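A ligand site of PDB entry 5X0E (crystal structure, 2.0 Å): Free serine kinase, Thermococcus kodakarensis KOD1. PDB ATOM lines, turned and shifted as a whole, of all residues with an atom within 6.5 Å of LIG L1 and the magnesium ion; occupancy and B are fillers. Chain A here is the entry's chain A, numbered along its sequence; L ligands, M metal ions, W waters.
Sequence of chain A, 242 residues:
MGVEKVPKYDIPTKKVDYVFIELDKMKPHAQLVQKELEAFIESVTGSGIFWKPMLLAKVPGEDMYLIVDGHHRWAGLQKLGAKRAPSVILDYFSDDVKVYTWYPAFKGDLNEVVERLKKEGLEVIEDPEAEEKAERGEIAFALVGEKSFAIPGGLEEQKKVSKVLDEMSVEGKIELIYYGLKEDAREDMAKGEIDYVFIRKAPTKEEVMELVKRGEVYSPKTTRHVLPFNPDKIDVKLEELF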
ATOM      1  N   GLY A   2      22.549  26.883 -10.056  1.00  0.00           N
ATOM      2  CA  GLY A   2      22.915  27.237 -11.454  1.00  0.00           C
ATOM      3  C   GLY A   2      24.052  28.216 -11.500  1.00  0.00           C
ATOM      4  O   GLY A   2      24.584  28.593 -10.455  1.00  0.00           O
ATOM      5  N   GLU A   4      23.907  31.404 -12.446  1.00  0.00           N
ATOM      6  CA  GLU A   4      23.535  32.813 -12.225  1.00  0.00           C
ATOM      7  C   GLU A   4      23.550  33.222 -10.744  1.00  0.00           C
ATOM      8  O   GLU A   4      23.150  32.454  -9.869  1.00  0.00           O
ATOM      9  CB  GLU A   4      22.163  33.120 -12.843  1.00  0.00           C
ATOM     10  CG  GLU A   4      22.136  33.008 -14.378  1.00  0.00           C
ATOM     11  CD  GLU A   4      20.735  32.792 -14.942  1.00  0.00           C
ATOM     12  OE1 GLU A   4      19.850  32.288 -14.225  1.00  0.00           O
ATOM     13  OE2 GLU A   4      20.515  33.118 -16.122  1.00  0.00           O
ATOM     14  N   LEU A  32      24.262  27.970 -25.134  1.00  0.00           N
ATOM     15  CA  LEU A  32      24.253  27.349 -23.787  1.00  0.00           C
ATOM     16  C   LEU A  32      25.589  27.419 -23.066  1.00  0.00           C
ATOM     17  O   LEU A  32      26.632  27.493 -23.704  1.00  0.00           O
ATOM     18  CB  LEU A  32      23.857  25.864 -23.911  1.00  0.00           C
ATOM     19  CG  LEU A  32      22.607  25.562 -24.744  1.00  0.00           C
ATOM     20  CD1 LEU A  32      22.268  24.085 -24.684  1.00  0.00           C
ATOM     21  CD2 LEU A  32      21.422  26.412 -24.279  1.00  0.00           C
ATOM     22  N   GLU A  36      25.422  25.081 -16.644  1.00  0.00           N
ATOM     23  CA  GLU A  36      24.008  25.415 -16.452  1.00  0.00           C
ATOM     24  C   GLU A  36      23.103  24.276 -16.982  1.00  0.00           C
ATOM     25  O   GLU A  36      22.136  23.876 -16.323  1.00  0.00           O
ATOM     26  CB  GLU A  36      23.680  26.738 -17.139  1.00  0.00           C
ATOM     27  CG  GLU A  36      22.273  27.285 -16.942  1.00  0.00           C
ATOM     28  CD  GLU A  36      22.077  28.029 -15.636  1.00  0.00           C
ATOM     29  OE1 GLU A  36      21.365  29.056 -15.657  1.00  0.00           O
ATOM     30  OE2 GLU A  36      22.626  27.605 -14.588  1.00  0.00           O
ATOM     31  N   LEU A  37      23.447  23.729 -18.142  1.00  0.00           N
ATOM     32  CA  LEU A  37      22.733  22.567 -18.707  1.00  0.00           C
ATOM     33  C   LEU A  37      22.818  21.330 -17.788  1.00  0.00           C
ATOM     34  O   LEU A  37      21.801  20.754 -17.405  1.00  0.00           O
ATOM     35  CB  LEU A  37      23.259  22.250 -20.124  1.00  0.00           C
ATOM     36  CG  LEU A  37      22.557  21.145 -20.924  1.00  0.00           C
ATOM     37  CD1 LEU A  37      21.044  21.310 -20.891  1.00  0.00           C
ATOM     38  CD2 LEU A  37      23.080  21.109 -22.350  1.00  0.00           C
ATOM     39  N   ALA A  39      23.646  21.116 -14.583  1.00  0.00           N
ATOM     40  CA  ALA A  39      22.988  21.371 -13.300  1.00  0.00           C
ATOM     41  C   ALA A  39      21.472  21.227 -13.382  1.00  0.00           C
ATOM     42  O   ALA A  39      20.858  20.660 -12.467  1.00  0.00           O
ATOM     43  CB  ALA A  39      23.381  22.757 -12.768  1.00  0.00           C
ATOM     44  N   PHE A  40      20.857  21.703 -14.463  1.00  0.00           N
ATOM     45  CA  PHE A  40      19.420  21.519 -14.659  1.00  0.00           C
ATOM     46  C   PHE A  40      19.059  20.034 -14.837  1.00  0.00           C
ATOM     47  O   PHE A  40      18.095  19.560 -14.235  1.00  0.00           O
ATOM     48  CB  PHE A  40      18.864  22.306 -15.851  1.00  0.00           C
ATOM     49  CG  PHE A  40      17.487  21.838 -16.252  1.00  0.00           C
ATOM     50  CD1 PHE A  40      16.395  22.115 -15.445  1.00  0.00           C
ATOM     51  CD2 PHE A  40      17.297  21.031 -17.372  1.00  0.00           C
ATOM     52  CE1 PHE A  40      15.125  21.652 -15.763  1.00  0.00           C
ATOM     53  CE2 PHE A  40      16.040  20.559 -17.694  1.00  0.00           C
ATOM     54  CZ  PHE A  40      14.954  20.872 -16.896  1.00  0.00           C
ATOM     55  N   SER A  43      19.407  18.318 -11.519  1.00  0.00           N
ATOM     56  CA  SER A  43      18.316  18.766 -10.625  1.00  0.00           C
ATOM     57  C   SER A  43      16.982  18.103 -10.957  1.00  0.00           C
ATOM     58  O   SER A  43      16.355  17.526 -10.075  1.00  0.00           O
ATOM     59  CB  SER A  43      18.152  20.282 -10.639  1.00  0.00           C
ATOM     60  OG  SER A  43      16.999  20.662  -9.913  1.00  0.00           O
ATOM     61  N   VAL A  44      16.560  18.172 -12.215  1.00  0.00           N
ATOM     62  CA  VAL A  44      15.233  17.698 -12.596  1.00  0.00           C
ATOM     63  C   VAL A  44      15.136  16.155 -12.535  1.00  0.00           C
ATOM     64  O   VAL A  44      14.124  15.622 -12.068  1.00  0.00           O
ATOM     65  CB  VAL A  44      14.763  18.267 -13.969  1.00  0.00           C
ATOM     66  CG1 VAL A  44      15.444  17.589 -15.145  1.00  0.00           C
ATOM     67  CG2 VAL A  44      13.251  18.179 -14.113  1.00  0.00           C
ATOM     68  N   THR A  45      16.181  15.457 -12.963  1.00  0.00           N
ATOM     69  CA  THR A  45      16.210  13.985 -12.878  1.00  0.00           C
ATOM     70  C   THR A  45      16.322  13.523 -11.429  1.00  0.00           C
ATOM     71  O   THR A  45      15.651  12.594 -11.040  1.00  0.00           O
ATOM     72  CB  THR A  45      17.322  13.344 -13.738  1.00  0.00           C
ATOM     73  OG1 THR A  45      18.604  13.892 -13.389  1.00  0.00           O
ATOM     74  CG2 THR A  45      17.049  13.568 -15.197  1.00  0.00           C
ATOM     75  N   SER A  47      15.497  15.254  -8.537  1.00  0.00           N
ATOM     76  CA  SER A  47      14.357  15.675  -7.721  1.00  0.00           C
ATOM     77  C   SER A  47      13.042  15.079  -8.201  1.00  0.00           C
ATOM     78  O   SER A  47      12.162  14.819  -7.393  1.00  0.00           O
ATOM     79  CB  SER A  47      14.263  17.207  -7.714  1.00  0.00           C
ATOM     80  OG  SER A  47      13.754  17.678  -8.942  1.00  0.00           O
ATOM     81  N   GLY A  48      12.912  14.882  -9.517  1.00  0.00           N
ATOM     82  CA  GLY A  48      11.676  14.423 -10.159  1.00  0.00           C
ATOM     83  C   GLY A  48      10.630  15.504 -10.358  1.00  0.00           C
ATOM     84  O   GLY A  48       9.521  15.224 -10.776  1.00  0.00           O
ATOM     85  N   ILE A  49      10.978  16.754 -10.064  1.00  0.00           N
ATOM     86  CA  ILE A  49      10.023  17.862 -10.096  1.00  0.00           C
ATOM     87  C   ILE A  49      10.609  18.972 -10.952  1.00  0.00           C
ATOM     88  O   ILE A  49      11.799  19.313 -10.830  1.00  0.00           O
ATOM     89  CB  ILE A  49       9.716  18.385  -8.666  1.00  0.00           C
ATOM     90  CG1 ILE A  49       8.973  17.311  -7.839  1.00  0.00           C
ATOM     91  CG2 ILE A  49       8.923  19.688  -8.719  1.00  0.00           C
ATOM     92  CD1 ILE A  49       7.531  17.053  -8.237  1.00  0.00           C
ATOM     93  N   PHE A  50       9.765  19.511 -11.825  1.00  0.00           N
ATOM     94  CA  PHE A  50      10.088  20.642 -12.676  1.00  0.00           C
ATOM     95  C   PHE A  50       9.309  21.815 -12.091  1.00  0.00           C
ATOM     96  O   PHE A  50       8.077  21.831 -12.171  1.00  0.00           O
ATOM     97  CB  PHE A  50       9.659  20.334 -14.097  1.00  0.00           C
ATOM     98  CG  PHE A  50       9.991  21.413 -15.097  1.00  0.00           C
ATOM     99  CD1 PHE A  50       9.142  22.502 -15.266  1.00  0.00           C
ATOM    100  CD2 PHE A  50      11.145  21.341 -15.844  1.00  0.00           C
ATOM    101  CE1 PHE A  50       9.449  23.494 -16.177  1.00  0.00           C
ATOM    102  CE2 PHE A  50      11.452  22.338 -16.768  1.00  0.00           C
ATOM    103  CZ  PHE A  50      10.597  23.414 -16.935  1.00  0.00           C
ATOM    104  N   TRP A  51      10.009  22.766 -11.477  1.00  0.00           N
ATOM    105  CA  TRP A  51       9.356  23.794 -10.608  1.00  0.00           C
ATOM    106  C   TRP A  51       9.349  25.244 -11.116  1.00  0.00           C
ATOM    107  O   TRP A  51       8.800  26.115 -10.444  1.00  0.00           O
ATOM    108  CB  TRP A  51       9.927  23.740  -9.173  1.00  0.00           C
ATOM    109  CG  TRP A  51      11.417  23.827  -9.112  1.00  0.00           C
ATOM    110  CD1 TRP A  51      12.285  22.789  -8.962  1.00  0.00           C
ATOM    111  CD2 TRP A  51      12.221  25.001  -9.231  1.00  0.00           C
ATOM    112  NE1 TRP A  51      13.577  23.237  -8.974  1.00  0.00           N
ATOM    113  CE2 TRP A  51      13.574  24.596  -9.125  1.00  0.00           C
ATOM    114  CE3 TRP A  51      11.942  26.366  -9.367  1.00  0.00           C
ATOM    115  CZ2 TRP A  51      14.643  25.493  -9.215  1.00  0.00           C
ATOM    116  CZ3 TRP A  51      13.017  27.279  -9.444  1.00  0.00           C
ATOM    117  CH2 TRP A  51      14.351  26.829  -9.362  1.00  0.00           C
ATOM    118  N   LYS A  52       9.924  25.501 -12.290  1.00  0.00           N
ATOM    119  CA  LYS A  52       9.977  26.874 -12.844  1.00  0.00           C
ATOM    120  C   LYS A  52       9.500  26.864 -14.297  1.00  0.00           C
ATOM    121  O   LYS A  52      10.145  26.256 -15.152  1.00  0.00           O
ATOM    122  CB  LYS A  52      11.399  27.441 -12.791  1.00  0.00           C
ATOM    123  CG  LYS A  52      11.483  28.909 -13.197  1.00  0.00           C
ATOM    124  CD  LYS A  52      12.921  29.425 -13.345  1.00  0.00           C
ATOM    125  CE  LYS A  52      13.547  29.770 -12.004  1.00  0.00           C
ATOM    126  NZ  LYS A  52      14.857  30.463 -12.182  1.00  0.00           N
ATOM    127  N   PRO A  53       8.397  27.562 -14.592  1.00  0.00           N
ATOM    128  CA  PRO A  53       7.928  27.549 -15.978  1.00  0.00           C
ATOM    129  C   PRO A  53       8.823  28.338 -16.914  1.00  0.00           C
ATOM    130  O   PRO A  53       9.429  29.357 -16.521  1.00  0.00           O
ATOM    131  CB  PRO A  53       6.545  28.193 -15.897  1.00  0.00           C
ATOM    132  CG  PRO A  53       6.681  29.122 -14.738  1.00  0.00           C
ATOM    133  CD  PRO A  53       7.498  28.356 -13.746  1.00  0.00           C
ATOM    134  N   MET A  54       8.938  27.858 -18.136  1.00  0.00           N
ATOM    135  CA  MET A  54       9.622  28.608 -19.188  1.00  0.00           C
ATOM    136  C   MET A  54       8.851  29.867 -19.522  1.00  0.00           C
ATOM    137  O   MET A  54       7.633  29.920 -19.301  1.00  0.00           O
ATOM    138  CB  MET A  54       9.788  27.741 -20.427  1.00  0.00           C
ATOM    139  CG  MET A  54      10.841  26.666 -20.218  1.00  0.00           C
ATOM    140  SD  MET A  54      11.147  25.800 -21.730  1.00  0.00           S
ATOM    141  CE  MET A  54      11.854  27.074 -22.784  1.00  0.00           C
ATOM    142  N   ASP A  69      13.049  33.045 -21.719  1.00  0.00           N
ATOM    143  CA  ASP A  69      13.914  32.511 -20.687  1.00  0.00           C
ATOM    144  C   ASP A  69      13.681  31.011 -20.585  1.00  0.00           C
ATOM    145  O   ASP A  69      12.516  30.577 -20.539  1.00  0.00           O
ATOM    146  CB  ASP A  69      13.572  33.175 -19.354  1.00  0.00           C
ATOM    147  CG  ASP A  69      14.435  32.682 -18.201  1.00  0.00           C
ATOM    148  OD1 ASP A  69      15.592  32.217 -18.385  1.00  0.00           O
ATOM    149  OD2 ASP A  69      13.940  32.747 -17.052  1.00  0.00           O
ATOM    150  N   GLY A  70      14.759  30.221 -20.534  1.00  0.00           N
ATOM    151  CA  GLY A  70      14.631  28.768 -20.515  1.00  0.00           C
ATOM    152  C   GLY A  70      15.389  27.944 -21.551  1.00  0.00           C
ATOM    153  O   GLY A  70      14.964  26.838 -21.865  1.00  0.00           O
ATOM    154  N   HIS A  71      16.523  28.422 -22.033  1.00  0.00           N
ATOM    155  CA  HIS A  71      17.314  27.687 -23.044  1.00  0.00           C
ATOM    156  C   HIS A  71      17.840  26.342 -22.565  1.00  0.00           C
ATOM    157  O   HIS A  71      17.876  25.380 -23.331  1.00  0.00           O
ATOM    158  CB  HIS A  71      18.484  28.523 -23.536  1.00  0.00           C
ATOM    159  CG  HIS A  71      18.056  29.668 -24.386  1.00  0.00           C
ATOM    160  ND1 HIS A  71      17.622  30.862 -23.851  1.00  0.00           N
ATOM    161  CD2 HIS A  71      17.894  29.764 -25.721  1.00  0.00           C
ATOM    162  CE1 HIS A  71      17.250  31.661 -24.830  1.00  0.00           C
ATOM    163  NE2 HIS A  71      17.400  31.021 -25.961  1.00  0.00           N
ATOM    164  N   HIS A  72      18.227  26.288 -21.293  1.00  0.00           N
ATOM    165  CA  HIS A  72      18.846  25.116 -20.721  1.00  0.00           C
ATOM    166  C   HIS A  72      17.810  24.107 -20.325  1.00  0.00           C
ATOM    167  O   HIS A  72      18.040  22.901 -20.476  1.00  0.00           O
ATOM    168  CB  HIS A  72      19.718  25.509 -19.540  1.00  0.00           C
ATOM    169  CG  HIS A  72      20.844  26.384 -19.941  1.00  0.00           C
ATOM    170  ND1 HIS A  72      20.700  27.730 -20.185  1.00  0.00           N
ATOM    171  CD2 HIS A  72      22.129  26.080 -20.256  1.00  0.00           C
ATOM    172  CE1 HIS A  72      21.855  28.229 -20.576  1.00  0.00           C
ATOM    173  NE2 HIS A  72      22.734  27.247 -20.631  1.00  0.00           N
ATOM    174  N   ARG A  73      16.696  24.590 -19.787  1.00  0.00           N
ATOM    175  CA  ARG A  73      15.533  23.723 -19.556  1.00  0.00           C
ATOM    176  C   ARG A  73      15.081  23.080 -20.882  1.00  0.00           C
ATOM    177  O   ARG A  73      14.852  21.872 -20.959  1.00  0.00           O
ATOM    178  CB  ARG A  73      14.387  24.498 -18.886  1.00  0.00           C
ATOM    179  CG  ARG A  73      14.555  24.616 -17.381  1.00  0.00           C
ATOM    180  CD  ARG A  73      13.639  25.666 -16.794  1.00  0.00           C
ATOM    181  NE  ARG A  73      14.081  27.019 -17.113  1.00  0.00           N
ATOM    182  CZ  ARG A  73      13.367  28.118 -16.926  1.00  0.00           C
ATOM    183  NH1 ARG A  73      12.118  28.059 -16.437  1.00  0.00           N
ATOM    184  NH2 ARG A  73      13.887  29.304 -17.247  1.00  0.00           N
ATOM    185  N   TRP A  74      15.020  23.888 -21.939  1.00  0.00           N
ATOM    186  CA  TRP A  74      14.591  23.401 -23.253  1.00  0.00           C
ATOM    187  C   TRP A  74      15.551  22.324 -23.790  1.00  0.00           C
ATOM    188  O   TRP A  74      15.132  21.221 -24.081  1.00  0.00           O
ATOM    189  CB  TRP A  74      14.431  24.572 -24.233  1.00  0.00           C
ATOM    190  CG  TRP A  74      14.272  24.209 -25.679  1.00  0.00           C
ATOM    191  CD1 TRP A  74      13.143  23.718 -26.311  1.00  0.00           C
ATOM    192  CD2 TRP A  74      15.268  24.377 -26.688  1.00  0.00           C
ATOM    193  NE1 TRP A  74      13.409  23.556 -27.651  1.00  0.00           N
ATOM    194  CE2 TRP A  74      14.695  23.949 -27.918  1.00  0.00           C
ATOM    195  CE3 TRP A  74      16.595  24.843 -26.687  1.00  0.00           C
ATOM    196  CZ2 TRP A  74      15.407  23.966 -29.123  1.00  0.00           C
ATOM    197  CZ3 TRP A  74      17.314  24.867 -27.882  1.00  0.00           C
ATOM    198  CH2 TRP A  74      16.705  24.431 -29.092  1.00  0.00           C
ATOM    199  N   TRP A 102      23.062  39.649 -18.802  1.00  0.00           N
ATOM    200  CA  TRP A 102      23.833  38.970 -17.762  1.00  0.00           C
ATOM    201  C   TRP A 102      25.297  39.164 -18.106  1.00  0.00           C
ATOM    202  O   TRP A 102      25.676  39.007 -19.280  1.00  0.00           O
ATOM    203  CB  TRP A 102      23.551  37.468 -17.744  1.00  0.00           C
ATOM    204  CG  TRP A 102      22.158  37.089 -17.356  1.00  0.00           C
ATOM    205  CD1 TRP A 102      21.111  36.849 -18.191  1.00  0.00           C
ATOM    206  CD2 TRP A 102      21.666  36.885 -16.028  1.00  0.00           C
ATOM    207  NE1 TRP A 102      19.993  36.529 -17.477  1.00  0.00           N
ATOM    208  CE2 TRP A 102      20.299  36.535 -16.144  1.00  0.00           C
ATOM    209  CE3 TRP A 102      22.232  36.965 -14.755  1.00  0.00           C
ATOM    210  CZ2 TRP A 102      19.491  36.268 -15.023  1.00  0.00           C
ATOM    211  CZ3 TRP A 102      21.431  36.677 -13.634  1.00  0.00           C
ATOM    212  CH2 TRP A 102      20.070  36.354 -13.793  1.00  0.00           C
ATOM    213  N   LYS A 221      23.296  33.754 -22.330  1.00  0.00           N
ATOM    214  CA  LYS A 221      22.830  34.689 -21.303  1.00  0.00           C
ATOM    215  C   LYS A 221      22.809  36.146 -21.748  1.00  0.00           C
ATOM    216  O   LYS A 221      22.917  37.047 -20.916  1.00  0.00           O
ATOM    217  CB  LYS A 221      23.659  34.547 -20.010  1.00  0.00           C
ATOM    218  CG  LYS A 221      23.728  33.144 -19.447  1.00  0.00           C
ATOM    219  CD  LYS A 221      22.360  32.655 -19.019  1.00  0.00           C
ATOM    220  CE  LYS A 221      22.433  31.345 -18.248  1.00  0.00           C
ATOM    221  NZ  LYS A 221      21.092  30.921 -17.735  1.00  0.00           N
HETATM  222  P1  LIG L   1      17.421  28.253 -18.254  1.00  0.00           P
HETATM  223  O1  LIG L   1      16.520  27.037 -18.375  1.00  0.00           O
HETATM  224  O2  LIG L   1      18.293  28.531 -19.455  1.00  0.00           O
HETATM  225  O3  LIG L   1      16.684  29.433 -17.712  1.00  0.00           O
HETATM  226  O4  LIG L   1      18.494  27.839 -17.120  1.00  0.00           O
HETATM  227  C1  LIG L   1      18.259  26.811 -16.163  1.00  0.00           C
HETATM  228  C2  LIG L   1      17.094  27.159 -15.238  1.00  0.00           C
HETATM  229  O5  LIG L   1      16.589  25.960 -14.680  1.00  0.00           O
HETATM  230  C3  LIG L   1      17.451  28.056 -14.057  1.00  0.00           C
HETATM  231  O6  LIG L   1      16.525  29.131 -14.026  1.00  0.00           O
HETATM  232  C4  LIG L   1      17.282  27.177 -12.834  1.00  0.00           C
HETATM  233  O7  LIG L   1      16.795  27.935 -11.737  1.00  0.00           O
HETATM  234  C5  LIG L   1      16.229  26.196 -13.318  1.00  0.00           C
HETATM  235  N1  LIG L   1      16.082  24.896 -12.623  1.00  0.00           N
HETATM  236  C6  LIG L   1      16.952  24.210 -11.843  1.00  0.00           C
HETATM  237  N2  LIG L   1      16.402  23.054 -11.405  1.00  0.00           N
HETATM  238  C7  LIG L   1      15.166  22.985 -11.946  1.00  0.00           C
HETATM  239  C8  LIG L   1      14.034  22.052 -11.906  1.00  0.00           C
HETATM  240  N3  LIG L   1      14.129  20.909 -11.209  1.00  0.00           N
HETATM  241  N4  LIG L   1      12.917  22.370 -12.614  1.00  0.00           N
HETATM  242  C9  LIG L   1      12.800  23.520 -13.331  1.00  0.00           C
HETATM  243  N5  LIG L   1      13.792  24.410 -13.386  1.00  0.00           N
HETATM  244  C10 LIG L   1      14.969  24.201 -12.735  1.00  0.00           C
HETATM  245  N1  LG2 L   2      17.174  34.727 -21.718  1.00  0.00           N
HETATM  246  C1  LG2 L   2      17.380  34.401 -20.280  1.00  0.00           C
HETATM  247  C2  LG2 L   2      18.849  34.122 -19.985  1.00  0.00           C
HETATM  248  O1  LG2 L   2      19.245  32.994 -20.759  1.00  0.00           O
HETATM  249  C3  LG2 L   2      16.822  35.514 -19.426  1.00  0.00           C
HETATM  250  O2  LG2 L   2      17.180  35.656 -18.255  1.00  0.00           O
HETATM  251  O3  LG2 L   2      15.985  36.287 -19.895  1.00  0.00           O
HETATM  252  P1  LG2 L   2      18.779  31.493 -20.359  1.00  0.00           P
HETATM  253  O4  LG2 L   2      18.488  31.591 -18.877  1.00  0.00           O
HETATM  254  O5  LG2 L   2      19.977  30.680 -20.780  1.00  0.00           O
HETATM  255  O6  LG2 L   2      17.569  31.259 -21.227  1.00  0.00           O
HETATM  256 MG    MG M   1      17.217  31.406 -17.363  1.00  0.00          MG
HETATM  257  O   HOH W   1      17.958  33.339 -16.602  1.00  0.00           O
HETATM  258  O   HOH W   2      15.862  31.418 -15.616  1.00  0.00           O
HETATM  259  O   HOH W   3      18.633  30.549 -16.068  1.00  0.00           O
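An oxygen (O4) of LIG L1 lies close to the side-chain carboxylate (OE1) of Glu 36, 3.4 Å away.
CD1 of Phe 40 touches C10 of LIG L1 (3.7 Å).
CA of Val 44 touches N3 of LIG L1 (3.7 Å).
Ser 47 touches LIG L1.
CA of Phe 50 touches N4 of LIG L1 (3.3 Å).
CA of Gly 70 touches O1 of LIG L1, 3.3 Å away.
Hydrophobic or aromatic side chains within 4 Å of LIG L1: Phe 40, Val 44, Phe 50, Trp 51 and His 72.
Of the 26 residues printed, 14 come within 4 Å of LIG L1.
The nearest printed residue that does not touch LIG L1 is Lys 221 (4.1 Å).
An oxygen (O2) of LIG L1 is in hydrogen-bond range of the backbone NH (N) of His 72.
ND1 of His 72 is in hydrogen-bond range of O2 of LIG L1 (2.6 Å).
The backbone NH (N) of Arg 73 lies within hydrogen-bond range of an oxygen (O1) of LIG L1.
The guanidinium group (NE) of Arg 73 is in salt-bridge range of an oxygen (O1) of LIG L1 (2.7 Å).
The side-chain amino group (NZ) of Lys 52 lies within hydrogen-bond range of an oxygen (O6) of LIG L1 (2.8 Å).
The backbone carbonyl oxygen of Ile 49 lies within hydrogen-bond range of a nitrogen (N3) of LIG L1 (2.8 Å).
N2 of LIG L1 lies within hydrogen-bond range of OG of Ser 43.
O2 of LIG L1 lies within hydrogen-bond range of N of His 71, at 3.1 Å.
The backbone NH (N) of Trp 51 is in hydrogen-bond range of a nitrogen (N4) of LIG L1.
A ring nitrogen (ND1) of His 72 sits close to an oxygen (O5) of LG2 L2, 3.1 Å away.
O6 of LG2 L2 is in hydrogen-bond range of N of His 71 (3.1 Å).
O6 of LG2 L2 lies within hydrogen-bond range of ND1 of His 71, 2.7 Å away.
An oxygen (O6) of LG2 L2 sits at hydrogen-bond distance from the backbone NH (N) of Gly 70 (3.1 Å).
An oxygen (O5) of LG2 L2 lies within salt-bridge range of the side-chain amino group (NZ) of Lys 221 (3.3 Å).
An oxygen (O2) of LG2 L2 sits at hydrogen-bond distance from the indole nitrogen (NE1) of Trp 102.
The guanidinium group (NH2) of Arg 73 lies within salt-bridge range of the side-chain carboxylate (OD2) of Asp 69, 3.4 Å away.
The backbone carbonyl oxygen of Lys 52 lies within hydrogen-bond range of the guanidinium group of Arg 73 (3.0 Å).
The guanidinium group (NH1) of Arg 73 is in hydrogen-bond range of the backbone carbonyl oxygen (O) of Pro 53.
N of Ile 49 lies within hydrogen-bond range of OG of Ser 47 (3.1 Å).
The side-chain hydroxyl of Ser 47 sits at hydrogen-bond distance from the backbone carbonyl oxygen of Ser 43 (2.8 Å).
The side-chain amino group (NZ) of Lys 221 is in salt-bridge range of the side-chain carboxylate (OE1) of Glu 36, 2.8 Å away.
OE2 of Glu 4 lies within salt-bridge range of NZ of Lys 221 (2.8 Å).
O of Lys 221 lies close to N of Trp 102, 3.4 Å away.
Water W2 lies within hydrogen-bond range of the side-chain carboxylate of Asp 69 (2.7 Å), an oxygen (O6) of LIG L1 (2.9 Å) and the guanidinium group of Arg 73 (3.3 Å).
Water W1 bridges the side-chain carboxylate of Glu 4 (2.6 Å) and an oxygen (O2) of LG2 L2 (3.0 Å).
O4 of LG2 L2 binds the magnesium ion (2.0 Å).
O3 of LIG L1 binds the magnesium ion (2.1 Å).
OD1 of Asp 69 binds the magnesium ion, at 2.1 Å.
Water W3 is bound to the magnesium ion.
Water W1 binds the magnesium ion, at 2.2 Å.
The magnesium ion is bound by water W2 (2.2 Å).
The magnesium ion has six donor atoms within binding distance.
Residues that only touch the magnesium ion: Glu 4 (3.9 Å), Lys 221 (3.9 Å) and Arg 73 (3.9 Å).
Along chain A the residues within 4 Å of the magnesium ion span positions 4 to 221.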
